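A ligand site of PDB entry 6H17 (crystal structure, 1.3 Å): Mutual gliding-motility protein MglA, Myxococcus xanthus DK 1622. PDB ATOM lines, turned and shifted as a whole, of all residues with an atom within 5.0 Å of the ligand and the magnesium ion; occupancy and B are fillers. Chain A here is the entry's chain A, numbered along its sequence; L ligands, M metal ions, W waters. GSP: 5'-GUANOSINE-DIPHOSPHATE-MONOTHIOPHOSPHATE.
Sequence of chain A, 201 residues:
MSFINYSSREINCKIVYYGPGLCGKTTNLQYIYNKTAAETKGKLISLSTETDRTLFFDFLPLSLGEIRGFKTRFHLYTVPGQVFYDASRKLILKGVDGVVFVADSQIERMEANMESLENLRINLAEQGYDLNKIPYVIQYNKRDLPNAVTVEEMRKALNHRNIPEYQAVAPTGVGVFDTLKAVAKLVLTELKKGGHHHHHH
Val 79 touches the ligand.
Pro 80 touches the ligand.
Gln 82 touches the ligand (OE1 to S1G, 3.96 Å).
Leu 145 touches the ligand (CD2 to N2, 3.6 Å).
CA of Val 169 touches O6 of the ligand (3.4 Å).
Pro 171 touches the ligand (CD to C5, 3.3 Å).
Hydrophobic or aromatic side chains within 4 Å of the ligand: Leu 22, Leu 145, Val 169, Ala 170 and Pro 171.
Of the 25 residues printed, 17 come within 4 Å of the ligand.
The nearest printed residue that does not touch the ligand is Gly 21 (4.1 Å).
An oxygen (O1B) of the ligand is in hydrogen-bond range of the backbone NH of Cys 23 (3.2 Å).
NZ of Lys 25 is in salt-bridge range of O1B of the ligand, at 2.8 Å.
OG1 of Thr 27 sits at hydrogen-bond distance from O1A of the ligand (2.7 Å).
The backbone NH (N) of Lys 25 sits at hydrogen-bond distance from an oxygen (O1B) of the ligand.
O6 of the ligand sits at hydrogen-bond distance from N of Lys 142 (3.2 Å).
The side-chain sulfur of Cys 23 sits at hydrogen-bond distance from an oxygen (O1B) of the ligand (3.6 Å).
ND2 of Asn 141 is in hydrogen-bond range of N7 of the ligand (3.0 Å).
The backbone NH (N) of Leu 22 sits at hydrogen-bond distance from an oxygen (O3B) of the ligand, 3.1 Å away.
The backbone NH (N) of Ala 170 is in hydrogen-bond range of an oxygen (O6) of the ligand, at 3.2 Å.
N of Thr 26 sits at hydrogen-bond distance from O1A of the ligand (3.4 Å).
N of Gly 24 is in hydrogen-bond range of O1B of the ligand, 3.0 Å away.
The backbone NH (N) of Gly 81 sits at hydrogen-bond distance from an oxygen (O3G) of the ligand, at 2.8 Å.
The backbone NH (N) of Thr 27 lies within hydrogen-bond range of an oxygen (O1A) of the ligand, at 2.9 Å.
The side-chain carboxylate of Asp 144 sits at hydrogen-bond distance from a nitrogen (N1) of the ligand, 2.8 Å away.
Water W6 lies within hydrogen-bond range of O of Val 79 and OG1 of Thr 78.
Water W2 bridges an oxygen (O2') of the ligand (2.7 Å) and the side-chain hydroxyl of Thr 27 (2.9 Å).
Water W8 lies within hydrogen-bond range of the backbone NH (N) of Gln 82 (3.0 Å), the backbone NH (N) of Gly 81 (3.2 Å) and a sulfur (S1G) of the ligand (3.3 Å).
The magnesium ion is bound by water W1 (2.0 Å).
The magnesium ion is bound by O2G of the ligand (2.1 Å).
The magnesium ion is bound by water W3 (2.1 Å).
An oxygen (O2B) of the ligand is bound to the magnesium ion (2.1 Å).
OG1 of Thr 26 binds the magnesium ion (2.1 Å).
Water W6 binds the magnesium ion (2.1 Å).
The magnesium ion has six donor atoms within binding distance.
Within 4 Å of the magnesium ion: Thr 26.
The nearest printed residue that does not touch the magnesium ion is Asp 58 (4.1 Å).
The side-chain amino group of Lys 25 lies within hydrogen-bond range of the side-chain sulfur of Cys 23, at 3.4 Å.
NZ of Lys 142 is in hydrogen-bond range of O of Leu 22 (2.8 Å).
The backbone carbonyl oxygen (O) of Gly 81 is in hydrogen-bond range of the backbone NH (N) of Gly 21 (3.4 Å).
NZ of Lys 25 is in hydrogen-bond range of O of Gly 19, 3.0 Å away.
The side-chain hydroxyl (OG1) of Thr 26 lies close to the side-chain carboxylate (OD2) of Asp 58.
O of Pro 20 lies within hydrogen-bond range of SG of Cys 23, at 3.2 Å.
The backbone carbonyl oxygen of Pro 20 lies within hydrogen-bond range of the side-chain amino group of Lys 25 (2.9 Å).
The backbone carbonyl oxygen of Ala 168 is in hydrogen-bond range of the backbone NH of Lys 142.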
ATOM      1  N   GLY A  19      -9.348  19.921  25.001  1.00  0.00           N
ATOM      2  CA  GLY A  19     -10.048  20.646  23.969  1.00  0.00           C
ATOM      3  C   GLY A  19     -10.497  22.001  24.468  1.00  0.00           C
ATOM      4  O   GLY A  19     -10.419  22.295  25.654  1.00  0.00           O
ATOM      5  N   PRO A  20     -11.000  22.832  23.573  1.00  0.00           N
ATOM      6  CA  PRO A  20     -11.259  24.242  23.915  1.00  0.00           C
ATOM      7  C   PRO A  20     -12.479  24.387  24.829  1.00  0.00           C
ATOM      8  O   PRO A  20     -13.215  23.445  25.098  1.00  0.00           O
ATOM      9  CB  PRO A  20     -11.449  24.895  22.552  1.00  0.00           C
ATOM     10  CG  PRO A  20     -11.957  23.798  21.698  1.00  0.00           C
ATOM     11  CD  PRO A  20     -11.227  22.554  22.146  1.00  0.00           C
ATOM     12  N   GLY A  21     -12.682  25.607  25.299  1.00  0.00           N
ATOM     13  CA  GLY A  21     -13.824  25.867  26.159  1.00  0.00           C
ATOM     14  C   GLY A  21     -15.117  25.395  25.567  1.00  0.00           C
ATOM     15  O   GLY A  21     -15.359  25.569  24.367  1.00  0.00           O
ATOM     16  N   LEU A  22     -15.956  24.771  26.382  1.00  0.00           N
ATOM     17  CA  LEU A  22     -17.324  24.393  26.027  1.00  0.00           C
ATOM     18  C   LEU A  22     -17.388  23.395  24.870  1.00  0.00           C
ATOM     19  O   LEU A  22     -18.441  23.273  24.241  1.00  0.00           O
ATOM     20  CB  LEU A  22     -18.202  25.634  25.764  1.00  0.00           C
ATOM     21  CG  LEU A  22     -18.328  26.578  26.970  1.00  0.00           C
ATOM     22  CD1 LEU A  22     -19.082  27.870  26.557  1.00  0.00           C
ATOM     23  CD2 LEU A  22     -18.997  25.917  28.160  1.00  0.00           C
ATOM     24  N   CYS A  23     -16.347  22.623  24.617  1.00  0.00           N
ATOM     25  CA  CYS A  23     -16.332  21.759  23.444  1.00  0.00           C
ATOM     26  C   CYS A  23     -17.028  20.418  23.640  1.00  0.00           C
ATOM     27  O   CYS A  23     -17.361  19.777  22.641  1.00  0.00           O
ATOM     28  CB  CYS A  23     -14.905  21.524  22.974  1.00  0.00           C
ATOM     29  SG  CYS A  23     -13.905  20.527  24.116  1.00  0.00           S
ATOM     30  N   GLY A  24     -17.248  19.980  24.872  1.00  0.00           N
ATOM     31  CA  GLY A  24     -17.943  18.741  25.149  1.00  0.00           C
ATOM     32  C   GLY A  24     -17.195  17.718  25.995  1.00  0.00           C
ATOM     33  O   GLY A  24     -17.595  16.548  26.015  1.00  0.00           O
ATOM     34  N   LYS A  25     -16.108  18.101  26.674  1.00  0.00           N
ATOM     35  CA  LYS A  25     -15.333  17.149  27.473  1.00  0.00           C
ATOM     36  C   LYS A  25     -16.151  16.596  28.639  1.00  0.00           C
ATOM     37  O   LYS A  25     -16.282  15.371  28.808  1.00  0.00           O
ATOM     38  CB  LYS A  25     -14.071  17.840  27.996  1.00  0.00           C
ATOM     39  CG  LYS A  25     -13.146  18.361  26.894  1.00  0.00           C
ATOM     40  CD  LYS A  25     -11.955  19.160  27.395  1.00  0.00           C
ATOM     41  CE  LYS A  25     -12.314  20.444  28.105  1.00  0.00           C
ATOM     42  NZ  LYS A  25     -12.882  21.502  27.235  1.00  0.00           N
ATOM     43  N   THR A  26     -16.698  17.490  29.467  1.00  0.00           N
ATOM     44  CA  THR A  26     -17.520  17.062  30.598  1.00  0.00           C
ATOM     45  C   THR A  26     -18.687  16.219  30.121  1.00  0.00           C
ATOM     46  O   THR A  26     -19.009  15.196  30.727  1.00  0.00           O
ATOM     47  CB  THR A  26     -17.988  18.297  31.367  1.00  0.00           C
ATOM     48  OG1 THR A  26     -16.835  18.940  31.950  1.00  0.00           O
ATOM     49  CG2 THR A  26     -18.990  17.923  32.478  1.00  0.00           C
ATOM     50  N   THR A  27     -19.316  16.611  29.006  1.00  0.00           N
ATOM     51  CA  THR A  27     -20.482  15.886  28.494  1.00  0.00           C
ATOM     52  C   THR A  27     -20.101  14.460  28.119  1.00  0.00           C
ATOM     53  O   THR A  27     -20.871  13.524  28.352  1.00  0.00           O
ATOM     54  CB  THR A  27     -21.026  16.619  27.271  1.00  0.00           C
ATOM     55  OG1 THR A  27     -21.446  17.930  27.635  1.00  0.00           O
ATOM     56  CG2 THR A  27     -22.250  15.915  26.690  1.00  0.00           C
ATOM     57  N   PHE A  56     -14.106  24.024  37.378  1.00  0.00           N
ATOM     58  CA  PHE A  56     -14.377  22.613  37.567  1.00  0.00           C
ATOM     59  C   PHE A  56     -13.725  21.768  36.491  1.00  0.00           C
ATOM     60  O   PHE A  56     -13.726  22.113  35.305  1.00  0.00           O
ATOM     61  CB  PHE A  56     -15.875  22.325  37.488  1.00  0.00           C
ATOM     62  CG  PHE A  56     -16.685  22.929  38.585  1.00  0.00           C
ATOM     63  CD1 PHE A  56     -16.610  22.434  39.884  1.00  0.00           C
ATOM     64  CD2 PHE A  56     -17.544  23.987  38.320  1.00  0.00           C
ATOM     65  CE1 PHE A  56     -17.366  22.995  40.895  1.00  0.00           C
ATOM     66  CE2 PHE A  56     -18.299  24.548  39.331  1.00  0.00           C
ATOM     67  CZ  PHE A  56     -18.205  24.056  40.620  1.00  0.00           C
ATOM     68  N   ASP A  58     -13.381  17.177  35.808  1.00  0.00           N
ATOM     69  CA  ASP A  58     -14.081  15.955  36.151  1.00  0.00           C
ATOM     70  C   ASP A  58     -13.103  14.804  36.326  1.00  0.00           C
ATOM     71  O   ASP A  58     -12.024  14.785  35.746  1.00  0.00           O
ATOM     72  CB  ASP A  58     -15.042  15.565  35.027  1.00  0.00           C
ATOM     73  CG  ASP A  58     -15.914  16.703  34.620  1.00  0.00           C
ATOM     74  OD1 ASP A  58     -16.826  17.060  35.392  1.00  0.00           O
ATOM     75  OD2 ASP A  58     -15.670  17.298  33.528  1.00  0.00           O
ATOM     76  N   THR A  78     -11.177  15.386  32.761  1.00  0.00           N
ATOM     77  CA  THR A  78     -11.249  16.508  31.823  1.00  0.00           C
ATOM     78  C   THR A  78     -10.385  17.638  32.351  1.00  0.00           C
ATOM     79  O   THR A  78      -9.833  17.563  33.452  1.00  0.00           O
ATOM     80  CB  THR A  78     -12.682  16.995  31.622  1.00  0.00           C
ATOM     81  OG1 THR A  78     -13.158  17.620  32.814  1.00  0.00           O
ATOM     82  CG2 THR A  78     -13.590  15.879  31.201  1.00  0.00           C
ATOM     83  N   VAL A  79     -10.245  18.680  31.539  1.00  0.00           N
ATOM     84  CA  VAL A  79      -9.520  19.884  31.912  1.00  0.00           C
ATOM     85  C   VAL A  79     -10.428  21.078  31.697  1.00  0.00           C
ATOM     86  O   VAL A  79     -11.417  20.986  30.953  1.00  0.00           O
ATOM     87  CB  VAL A  79      -8.224  20.067  31.090  1.00  0.00           C
ATOM     88  CG1 VAL A  79      -7.343  18.822  31.186  1.00  0.00           C
ATOM     89  CG2 VAL A  79      -8.525  20.415  29.651  1.00  0.00           C
ATOM     90  N   PRO A  80     -10.092  22.235  32.287  1.00  0.00           N
ATOM     91  CA  PRO A  80     -10.783  23.479  31.905  1.00  0.00           C
ATOM     92  C   PRO A  80     -10.190  23.996  30.615  1.00  0.00           C
ATOM     93  O   PRO A  80      -8.998  24.306  30.542  1.00  0.00           O
ATOM     94  CB  PRO A  80     -10.523  24.411  33.092  1.00  0.00           C
ATOM     95  CG  PRO A  80      -9.391  23.816  33.837  1.00  0.00           C
ATOM     96  CD  PRO A  80      -9.191  22.403  33.438  1.00  0.00           C
ATOM     97  N   GLY A  81     -10.994  24.044  29.566  1.00  0.00           N
ATOM     98  CA  GLY A  81     -10.509  24.357  28.244  1.00  0.00           C
ATOM     99  C   GLY A  81     -10.388  25.805  27.888  1.00  0.00           C
ATOM    100  O   GLY A  81      -9.727  26.134  26.888  1.00  0.00           O
ATOM    101  N   GLN A  82     -11.003  26.711  28.643  1.00  0.00           N
ATOM    102  CA  GLN A  82     -10.904  28.115  28.293  1.00  0.00           C
ATOM    103  C   GLN A  82      -9.448  28.579  28.376  1.00  0.00           C
ATOM    104  O   GLN A  82      -8.699  28.146  29.268  1.00  0.00           O
ATOM    105  CB  GLN A  82     -11.779  28.946  29.211  1.00  0.00           C
ATOM    106  CG  GLN A  82     -13.286  28.758  29.015  1.00  0.00           C
ATOM    107  CD  GLN A  82     -14.083  29.462  30.093  1.00  0.00           C
ATOM    108  OE1 GLN A  82     -14.367  28.894  31.142  1.00  0.00           O
ATOM    109  NE2 GLN A  82     -14.435  30.711  29.836  1.00  0.00           N
ATOM    110  N   ASN A 141     -16.760  16.571  17.745  1.00  0.00           N
ATOM    111  CA  ASN A 141     -18.010  16.632  18.487  1.00  0.00           C
ATOM    112  C   ASN A 141     -18.930  17.695  17.911  1.00  0.00           C
ATOM    113  O   ASN A 141     -18.541  18.539  17.088  1.00  0.00           O
ATOM    114  CB  ASN A 141     -17.715  16.869  19.976  1.00  0.00           C
ATOM    115  CG  ASN A 141     -18.911  16.645  20.846  1.00  0.00           C
ATOM    116  OD1 ASN A 141     -19.709  15.738  20.611  1.00  0.00           O
ATOM    117  ND2 ASN A 141     -19.060  17.468  21.871  1.00  0.00           N
ATOM    118  N   LYS A 142     -20.181  17.652  18.333  1.00  0.00           N
ATOM    119  CA  LYS A 142     -21.227  18.595  17.895  1.00  0.00           C
ATOM    120  C   LYS A 142     -21.573  18.434  16.414  1.00  0.00           C
ATOM    121  O   LYS A 142     -21.885  19.401  15.716  1.00  0.00           O
ATOM    122  CB  LYS A 142     -20.924  20.056  18.253  1.00  0.00           C
ATOM    123  CG  LYS A 142     -20.382  20.235  19.676  1.00  0.00           C
ATOM    124  CD  LYS A 142     -20.679  21.621  20.225  1.00  0.00           C
ATOM    125  CE  LYS A 142     -20.105  21.771  21.624  1.00  0.00           C
ATOM    126  NZ  LYS A 142     -20.177  23.196  22.080  1.00  0.00           N
ATOM    127  N   ARG A 143     -21.604  17.183  15.942  1.00  0.00           N
ATOM    128  CA  ARG A 143     -21.967  16.925  14.552  1.00  0.00           C
ATOM    129  C   ARG A 143     -23.422  17.262  14.254  1.00  0.00           C
ATOM    130  O   ARG A 143     -23.784  17.359  13.073  1.00  0.00           O
ATOM    131  CB  ARG A 143     -21.723  15.458  14.173  1.00  0.00           C
ATOM    132  CG  ARG A 143     -20.295  14.964  14.344  1.00  0.00           C
ATOM    133  CD  ARG A 143     -19.282  15.832  13.644  1.00  0.00           C
ATOM    134  NE  ARG A 143     -19.660  16.078  12.252  1.00  0.00           N
ATOM    135  CZ  ARG A 143     -19.203  17.071  11.506  1.00  0.00           C
ATOM    136  NH1 ARG A 143     -18.296  17.899  11.984  1.00  0.00           N
ATOM    137  NH2 ARG A 143     -19.620  17.206  10.257  1.00  0.00           N
ATOM    138  N   ASP A 144     -24.244  17.460  15.281  1.00  0.00           N
ATOM    139  CA  ASP A 144     -25.657  17.742  15.112  1.00  0.00           C
ATOM    140  C   ASP A 144     -25.938  19.182  14.718  1.00  0.00           C
ATOM    141  O   ASP A 144     -27.056  19.494  14.310  1.00  0.00           O
ATOM    142  CB  ASP A 144     -26.395  17.461  16.432  1.00  0.00           C
ATOM    143  CG  ASP A 144     -25.867  18.290  17.589  1.00  0.00           C
ATOM    144  OD1 ASP A 144     -26.673  19.004  18.224  1.00  0.00           O
ATOM    145  OD2 ASP A 144     -24.653  18.234  17.878  1.00  0.00           O
ATOM    146  N   LEU A 145     -24.960  20.071  14.824  1.00  0.00           N
ATOM    147  CA  LEU A 145     -25.238  21.487  14.669  1.00  0.00           C
ATOM    148  C   LEU A 145     -25.148  21.919  13.198  1.00  0.00           C
ATOM    149  O   LEU A 145     -24.304  21.425  12.451  1.00  0.00           O
ATOM    150  CB  LEU A 145     -24.285  22.319  15.520  1.00  0.00           C
ATOM    151  CG  LEU A 145     -24.531  22.168  17.029  1.00  0.00           C
ATOM    152  CD1 LEU A 145     -23.553  22.989  17.827  1.00  0.00           C
ATOM    153  CD2 LEU A 145     -25.966  22.541  17.363  1.00  0.00           C
ATOM    154  N   ALA A 168     -18.877  12.656  16.798  1.00  0.00           N
ATOM    155  CA  ALA A 168     -19.637  12.533  18.038  1.00  0.00           C
ATOM    156  C   ALA A 168     -20.736  13.573  18.162  1.00  0.00           C
ATOM    157  O   ALA A 168     -20.675  14.679  17.592  1.00  0.00           O
ATOM    158  CB  ALA A 168     -18.742  12.623  19.255  1.00  0.00           C
ATOM    159  N   VAL A 169     -21.754  13.189  18.949  1.00  0.00           N
ATOM    160  CA  VAL A 169     -22.771  14.093  19.486  1.00  0.00           C
ATOM    161  C   VAL A 169     -22.830  13.718  20.976  1.00  0.00           C
ATOM    162  O   VAL A 169     -23.595  12.831  21.374  1.00  0.00           O
ATOM    163  CB  VAL A 169     -24.133  13.950  18.810  1.00  0.00           C
ATOM    164  CG1 VAL A 169     -25.104  14.978  19.374  1.00  0.00           C
ATOM    165  CG2 VAL A 169     -24.012  14.114  17.325  1.00  0.00           C
ATOM    166  N   ALA A 170     -21.982  14.346  21.781  1.00  0.00           N
ATOM    167  CA  ALA A 170     -21.767  13.804  23.114  1.00  0.00           C
ATOM    168  C   ALA A 170     -23.041  13.709  23.955  1.00  0.00           C
ATOM    169  O   ALA A 170     -23.196  12.712  24.680  1.00  0.00           O
ATOM    170  CB  ALA A 170     -20.655  14.587  23.837  1.00  0.00           C
ATOM    171  N   PRO A 171     -23.976  14.676  23.935  1.00  0.00           N
ATOM    172  CA  PRO A 171     -25.145  14.570  24.820  1.00  0.00           C
ATOM    173  C   PRO A 171     -26.008  13.362  24.533  1.00  0.00           C
ATOM    174  O   PRO A 171     -26.685  12.863  25.443  1.00  0.00           O
ATOM    175  CB  PRO A 171     -25.898  15.882  24.575  1.00  0.00           C
ATOM    176  CG  PRO A 171     -24.827  16.828  24.111  1.00  0.00           C
ATOM    177  CD  PRO A 171     -23.896  15.987  23.269  1.00  0.00           C
HETATM  178  PG  GSP L   1     -15.025  23.464  29.800  1.00  0.00           P
HETATM  179  O3B GSP L   1     -16.110  22.813  28.739  1.00  0.00           O
HETATM  180  S1G GSP L   1     -15.399  25.299  29.852  1.00  0.00           S
HETATM  181  O2G GSP L   1     -15.245  22.704  31.131  1.00  0.00           O
HETATM  182  O3G GSP L   1     -13.643  23.126  29.233  1.00  0.00           O
HETATM  183  PB  GSP L   1     -16.451  21.316  28.354  1.00  0.00           P
HETATM  184  O1B GSP L   1     -15.614  20.867  27.218  1.00  0.00           O
HETATM  185  O2B GSP L   1     -16.431  20.446  29.562  1.00  0.00           O
HETATM  186  PA  GSP L   1     -19.293  20.779  28.277  1.00  0.00           P
HETATM  187  O1A GSP L   1     -19.186  19.338  28.125  1.00  0.00           O
HETATM  188  O2A GSP L   1     -19.701  21.315  29.579  1.00  0.00           O
HETATM  189  O3A GSP L   1     -17.953  21.492  27.810  1.00  0.00           O
HETATM  190  O5' GSP L   1     -20.287  21.275  27.127  1.00  0.00           O
HETATM  191  C5' GSP L   1     -20.557  22.656  26.949  1.00  0.00           C
HETATM  192  C4' GSP L   1     -21.920  22.848  26.312  1.00  0.00           C
HETATM  193  O4' GSP L   1     -21.944  22.242  25.005  1.00  0.00           O
HETATM  194  C3' GSP L   1     -23.017  22.183  27.104  1.00  0.00           C
HETATM  195  O3' GSP L   1     -24.185  23.000  27.080  1.00  0.00           O
HETATM  196  C2' GSP L   1     -23.307  20.866  26.382  1.00  0.00           C
HETATM  197  O2' GSP L   1     -24.597  20.372  26.528  1.00  0.00           O
HETATM  198  C1' GSP L   1     -22.999  21.304  24.944  1.00  0.00           C
HETATM  199  N9  GSP L   1     -22.615  20.209  24.058  1.00  0.00           N
HETATM  200  C8  GSP L   1     -21.646  19.296  24.300  1.00  0.00           C
HETATM  201  N7  GSP L   1     -21.572  18.420  23.263  1.00  0.00           N
HETATM  202  C5  GSP L   1     -22.522  18.809  22.361  1.00  0.00           C
HETATM  203  C6  GSP L   1     -22.915  18.301  21.119  1.00  0.00           C
HETATM  204  O6  GSP L   1     -22.410  17.293  20.557  1.00  0.00           O
HETATM  205  N1  GSP L   1     -23.936  18.939  20.496  1.00  0.00           N
HETATM  206  C2  GSP L   1     -24.539  20.057  21.024  1.00  0.00           C
HETATM  207  N2  GSP L   1     -25.506  20.643  20.344  1.00  0.00           N
HETATM  208  N3  GSP L   1     -24.177  20.572  22.216  1.00  0.00           N
HETATM  209  C4  GSP L   1     -23.183  19.926  22.854  1.00  0.00           C
HETATM  210 MG    MG M   1     -16.068  20.869  31.589  1.00  0.00          MG
HETATM  211  O   HOH W   1     -15.870  21.110  33.609  1.00  0.00           O
HETATM  212  O   HOH W   2     -24.158  18.519  28.419  1.00  0.00           O
HETATM  213  O   HOH W   3     -18.010  21.617  31.732  1.00  0.00           O
HETATM  214  O   HOH W   4     -20.710  23.874  30.687  1.00  0.00           O
HETATM  215  O   HOH W   5     -26.547  23.384  20.958  1.00  0.00           O
HETATM  216  O   HOH W   6     -14.100  20.082  31.477  1.00  0.00           O
HETATM  217  O   HOH W   7     -18.070  24.790  31.671  1.00  0.00           O
HETATM  218  O   HOH W   8     -12.602  26.298  31.181  1.00  0.00           O
HETATM  219  O   HOH W   9     -14.202  24.057  33.326  1.00  0.00           O
HETATM  220  O   HOH W  10     -21.782  20.304  31.125  1.00  0.00           O
